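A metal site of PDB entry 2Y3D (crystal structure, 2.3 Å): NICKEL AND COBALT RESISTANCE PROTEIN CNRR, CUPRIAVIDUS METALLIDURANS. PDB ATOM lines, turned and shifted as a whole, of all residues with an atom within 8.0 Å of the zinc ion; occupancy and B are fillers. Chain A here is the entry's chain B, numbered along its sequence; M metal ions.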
ATOM      1  N   HIS A  12     -29.264 -16.048  25.266  1.00  0.00           N
ATOM      2  CA  HIS A  12     -28.052 -16.804  25.491  1.00  0.00           C
ATOM      3  C   HIS A  12     -28.025 -18.060  24.625  1.00  0.00           C
ATOM      4  O   HIS A  12     -27.043 -18.345  23.972  1.00  0.00           O
ATOM      5  CB  HIS A  12     -27.933 -17.163  26.972  1.00  0.00           C
ATOM      6  CG  HIS A  12     -26.755 -18.025  27.308  1.00  0.00           C
ATOM      7  ND1 HIS A  12     -26.896 -19.262  27.922  1.00  0.00           N
ATOM      8  CD2 HIS A  12     -25.425 -17.837  27.147  1.00  0.00           C
ATOM      9  CE1 HIS A  12     -25.701 -19.781  28.109  1.00  0.00           C
ATOM     10  NE2 HIS A  12     -24.796 -18.936  27.648  1.00  0.00           N
ATOM     11  N   GLU A  13     -29.146 -18.780  24.598  1.00  0.00           N
ATOM     12  CA  GLU A  13     -29.176 -20.047  23.883  1.00  0.00           C
ATOM     13  C   GLU A  13     -29.192 -19.834  22.388  1.00  0.00           C
ATOM     14  O   GLU A  13     -28.666 -20.646  21.635  1.00  0.00           O
ATOM     15  CB  GLU A  13     -30.385 -20.889  24.309  1.00  0.00           C
ATOM     16  CG  GLU A  13     -31.049 -20.404  25.577  1.00  0.00           C
ATOM     17  CD  GLU A  13     -31.637 -21.537  26.389  1.00  0.00           C
ATOM     18  OE1 GLU A  13     -32.738 -22.015  26.031  1.00  0.00           O
ATOM     19  OE2 GLU A  13     -30.972 -21.948  27.377  1.00  0.00           O
ATOM     20  N   LEU A  15     -27.725 -17.415  20.768  1.00  0.00           N
ATOM     21  CA  LEU A  15     -26.399 -17.038  20.303  1.00  0.00           C
ATOM     22  C   LEU A  15     -25.467 -18.232  20.279  1.00  0.00           C
ATOM     23  O   LEU A  15     -24.622 -18.345  19.401  1.00  0.00           O
ATOM     24  CB  LEU A  15     -25.844 -15.872  21.104  1.00  0.00           C
ATOM     25  CG  LEU A  15     -26.516 -14.599  20.587  1.00  0.00           C
ATOM     26  CD1 LEU A  15     -26.465 -13.488  21.602  1.00  0.00           C
ATOM     27  CD2 LEU A  15     -25.882 -14.172  19.249  1.00  0.00           C
ATOM     28  N   HIS A  16     -25.650 -19.152  21.224  1.00  0.00           N
ATOM     29  CA  HIS A  16     -24.872 -20.395  21.193  1.00  0.00           C
ATOM     30  C   HIS A  16     -25.123 -21.174  19.903  1.00  0.00           C
ATOM     31  O   HIS A  16     -24.218 -21.803  19.377  1.00  0.00           O
ATOM     32  CB  HIS A  16     -25.141 -21.264  22.426  1.00  0.00           C
ATOM     33  CG  HIS A  16     -24.244 -20.965  23.591  1.00  0.00           C
ATOM     34  ND1 HIS A  16     -22.947 -21.442  23.661  1.00  0.00           N
ATOM     35  CD2 HIS A  16     -24.446 -20.261  24.714  1.00  0.00           C
ATOM     36  CE1 HIS A  16     -22.402 -21.030  24.790  1.00  0.00           C
ATOM     37  NE2 HIS A  16     -23.282 -20.319  25.460  1.00  0.00           N
ATOM     38  N   LEU A  29     -15.471 -25.011  23.922  1.00  0.00           N
ATOM     39  CA  LEU A  29     -16.442 -23.997  24.292  1.00  0.00           C
ATOM     40  C   LEU A  29     -17.199 -24.402  25.560  1.00  0.00           C
ATOM     41  O   LEU A  29     -17.444 -23.569  26.443  1.00  0.00           O
ATOM     42  CB  LEU A  29     -17.411 -23.730  23.132  1.00  0.00           C
ATOM     43  CG  LEU A  29     -18.499 -22.657  23.338  1.00  0.00           C
ATOM     44  CD1 LEU A  29     -17.908 -21.249  23.284  1.00  0.00           C
ATOM     45  CD2 LEU A  29     -19.622 -22.801  22.325  1.00  0.00           C
ATOM     46  N   LYS A  32     -15.169 -23.824  28.544  1.00  0.00           N
ATOM     47  CA  LYS A  32     -15.107 -22.395  28.836  1.00  0.00           C
ATOM     48  C   LYS A  32     -16.412 -21.824  29.437  1.00  0.00           C
ATOM     49  O   LYS A  32     -16.430 -20.707  29.970  1.00  0.00           O
ATOM     50  CB  LYS A  32     -14.733 -21.622  27.577  1.00  0.00           C
ATOM     51  CG  LYS A  32     -13.344 -21.923  27.041  1.00  0.00           C
ATOM     52  CD  LYS A  32     -12.348 -20.946  27.613  1.00  0.00           C
ATOM     53  CE  LYS A  32     -10.961 -21.141  27.025  1.00  0.00           C
ATOM     54  NZ  LYS A  32      -9.958 -20.308  27.745  1.00  0.00           N
ATOM     55  N   GLU A  33     -17.499 -22.598  29.347  1.00  0.00           N
ATOM     56  CA  GLU A  33     -18.831 -22.167  29.787  1.00  0.00           C
ATOM     57  C   GLU A  33     -18.941 -21.927  31.281  1.00  0.00           C
ATOM     58  O   GLU A  33     -19.722 -21.086  31.728  1.00  0.00           O
ATOM     59  CB  GLU A  33     -19.876 -23.229  29.445  1.00  0.00           C
ATOM     60  CG  GLU A  33     -20.695 -22.968  28.199  1.00  0.00           C
ATOM     61  CD  GLU A  33     -21.198 -21.543  28.133  1.00  0.00           C
ATOM     62  OE1 GLU A  33     -22.154 -21.196  28.876  1.00  0.00           O
ATOM     63  OE2 GLU A  33     -20.617 -20.770  27.319  1.00  0.00           O
ATOM     64  N   ASP A  34     -18.171 -22.690  32.057  1.00  0.00           N
ATOM     65  CA  ASP A  34     -18.381 -22.781  33.500  1.00  0.00           C
ATOM     66  C   ASP A  34     -18.195 -21.456  34.226  1.00  0.00           C
ATOM     67  O   ASP A  34     -18.918 -21.178  35.183  1.00  0.00           O
ATOM     68  CB  ASP A  34     -17.542 -23.917  34.091  1.00  0.00           C
ATOM     69  CG  ASP A  34     -17.900 -25.281  33.481  1.00  0.00           C
ATOM     70  OD1 ASP A  34     -19.041 -25.438  32.975  1.00  0.00           O
ATOM     71  OD2 ASP A  34     -17.044 -26.201  33.481  1.00  0.00           O
ATOM     72  N   PHE A  36     -19.071 -18.540  33.130  1.00  0.00           N
ATOM     73  CA  PHE A  36     -20.315 -17.805  32.979  1.00  0.00           C
ATOM     74  C   PHE A  36     -21.477 -18.520  33.653  1.00  0.00           C
ATOM     75  O   PHE A  36     -22.368 -17.861  34.207  1.00  0.00           O
ATOM     76  CB  PHE A  36     -20.665 -17.514  31.512  1.00  0.00           C
ATOM     77  CG  PHE A  36     -22.079 -17.053  31.334  1.00  0.00           C
ATOM     78  CD1 PHE A  36     -22.439 -15.755  31.651  1.00  0.00           C
ATOM     79  CD2 PHE A  36     -23.051 -17.920  30.874  1.00  0.00           C
ATOM     80  CE1 PHE A  36     -23.740 -15.328  31.501  1.00  0.00           C
ATOM     81  CE2 PHE A  36     -24.365 -17.508  30.714  1.00  0.00           C
ATOM     82  CZ  PHE A  36     -24.713 -16.204  31.036  1.00  0.00           C
ATOM     83  N   ALA A  37     -21.496 -19.853  33.583  1.00  0.00           N
ATOM     84  CA  ALA A  37     -22.617 -20.609  34.145  1.00  0.00           C
ATOM     85  C   ALA A  37     -22.766 -20.273  35.621  1.00  0.00           C
ATOM     86  O   ALA A  37     -23.876 -20.033  36.092  1.00  0.00           O
ATOM     87  CB  ALA A  37     -22.433 -22.096  33.952  1.00  0.00           C
ATOM     88  N   ARG A  40     -23.842 -16.478  36.628  1.00  0.00           N
ATOM     89  CA  ARG A  40     -25.236 -16.593  36.193  1.00  0.00           C
ATOM     90  C   ARG A  40     -26.076 -17.219  37.275  1.00  0.00           C
ATOM     91  O   ARG A  40     -27.203 -16.774  37.525  1.00  0.00           O
ATOM     92  CB  ARG A  40     -25.366 -17.422  34.915  1.00  0.00           C
ATOM     93  CG  ARG A  40     -26.789 -17.554  34.411  1.00  0.00           C
ATOM     94  CD  ARG A  40     -26.903 -18.323  33.096  1.00  0.00           C
ATOM     95  NE  ARG A  40     -26.512 -19.727  33.206  1.00  0.00           N
ATOM     96  CZ  ARG A  40     -27.310 -20.705  33.647  1.00  0.00           C
ATOM     97  NH1 ARG A  40     -28.561 -20.448  34.021  1.00  0.00           N
ATOM     98  NH2 ARG A  40     -26.841 -21.962  33.706  1.00  0.00           N
ATOM     99  N   THR A  86     -25.112 -11.602  30.815  1.00  0.00           N
ATOM    100  CA  THR A  86     -25.324 -12.322  29.572  1.00  0.00           C
ATOM    101  C   THR A  86     -24.557 -11.630  28.429  1.00  0.00           C
ATOM    102  O   THR A  86     -23.842 -12.278  27.690  1.00  0.00           O
ATOM    103  CB  THR A  86     -26.830 -12.486  29.228  1.00  0.00           C
ATOM    104  OG1 THR A  86     -27.482 -13.207  30.277  1.00  0.00           O
ATOM    105  CG2 THR A  86     -27.024 -13.250  27.911  1.00  0.00           C
ATOM    106  N   HIS A  89     -20.754 -12.016  28.507  1.00  0.00           N
ATOM    107  CA  HIS A  89     -20.415 -13.364  28.073  1.00  0.00           C
ATOM    108  C   HIS A  89     -20.619 -13.545  26.568  1.00  0.00           C
ATOM    109  O   HIS A  89     -19.892 -14.286  25.922  1.00  0.00           O
ATOM    110  CB  HIS A  89     -21.208 -14.393  28.905  1.00  0.00           C
ATOM    111  CG  HIS A  89     -21.273 -15.772  28.311  1.00  0.00           C
ATOM    112  ND1 HIS A  89     -20.178 -16.598  28.178  1.00  0.00           N
ATOM    113  CD2 HIS A  89     -22.339 -16.504  27.863  1.00  0.00           C
ATOM    114  CE1 HIS A  89     -20.546 -17.745  27.635  1.00  0.00           C
ATOM    115  NE2 HIS A  89     -21.858 -17.713  27.442  1.00  0.00           N
ATOM    116  N   VAL A  90     -21.586 -12.843  26.006  1.00  0.00           N
ATOM    117  CA  VAL A  90     -21.827 -12.929  24.573  1.00  0.00           C
ATOM    118  C   VAL A  90     -20.725 -12.265  23.752  1.00  0.00           C
ATOM    119  O   VAL A  90     -20.346 -12.752  22.675  1.00  0.00           O
ATOM    120  CB  VAL A  90     -23.199 -12.353  24.199  1.00  0.00           C
ATOM    121  CG1 VAL A  90     -23.252 -12.026  22.716  1.00  0.00           C
ATOM    122  CG2 VAL A  90     -24.264 -13.360  24.564  1.00  0.00           C
ATOM    123  N   MET A  93     -17.669 -14.552  23.722  1.00  0.00           N
ATOM    124  CA  MET A  93     -17.824 -15.613  22.733  1.00  0.00           C
ATOM    125  C   MET A  93     -17.610 -15.071  21.313  1.00  0.00           C
ATOM    126  O   MET A  93     -17.219 -15.807  20.413  1.00  0.00           O
ATOM    127  CB  MET A  93     -19.209 -16.257  22.848  1.00  0.00           C
ATOM    128  CG  MET A  93     -19.447 -17.005  24.145  1.00  0.00           C
ATOM    129  SD  MET A  93     -20.880 -18.082  24.080  1.00  0.00           S
ATOM    130  CE  MET A  93     -22.216 -16.896  24.236  1.00  0.00           C
ATOM    131  N   TYR A 105     -23.305 -13.616  13.477  1.00  0.00           N
ATOM    132  CA  TYR A 105     -23.478 -13.581  14.930  1.00  0.00           C
ATOM    133  C   TYR A 105     -24.028 -12.242  15.410  1.00  0.00           C
ATOM    134  O   TYR A 105     -24.907 -12.209  16.255  1.00  0.00           O
ATOM    135  CB  TYR A 105     -22.133 -13.835  15.596  1.00  0.00           C
ATOM    136  CG  TYR A 105     -22.121 -13.969  17.095  1.00  0.00           C
ATOM    137  CD1 TYR A 105     -22.372 -15.195  17.703  1.00  0.00           C
ATOM    138  CD2 TYR A 105     -21.793 -12.896  17.910  1.00  0.00           C
ATOM    139  CE1 TYR A 105     -22.329 -15.336  19.070  1.00  0.00           C
ATOM    140  CE2 TYR A 105     -21.728 -13.028  19.273  1.00  0.00           C
ATOM    141  CZ  TYR A 105     -21.998 -14.259  19.853  1.00  0.00           C
ATOM    142  OH  TYR A 105     -21.944 -14.398  21.212  1.00  0.00           O
HETATM  143 ZN    ZN M   1     -22.800 -19.434  27.203  1.00  0.00          ZN
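The zinc ion is bound by NE2 of His 89 (2.0 Å), NE2 of His 16 (2.0 Å), NE2 of His 12 (2.1 Å), OE1 of Glu 33 (2.5 Å) and OE2 of Glu 33 (2.6 Å).
The zinc ion has five donor atoms within binding distance.
The side-chain sulfur (SD) of Met 93 sits close to a ring nitrogen (NE2) of His 89, at 3.5 Å.
The side-chain sulfur of Met 93 lies close to a ring nitrogen (NE2) of His 16, at 3.6 Å.
Residues that only touch the zinc ion: Phe 36 and Met 93.
Of the 16 residues printed, 6 come within 4 Å of the zinc ion.
The nearest printed residue that does not touch the zinc ion is Ala 37 (6.5 Å).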
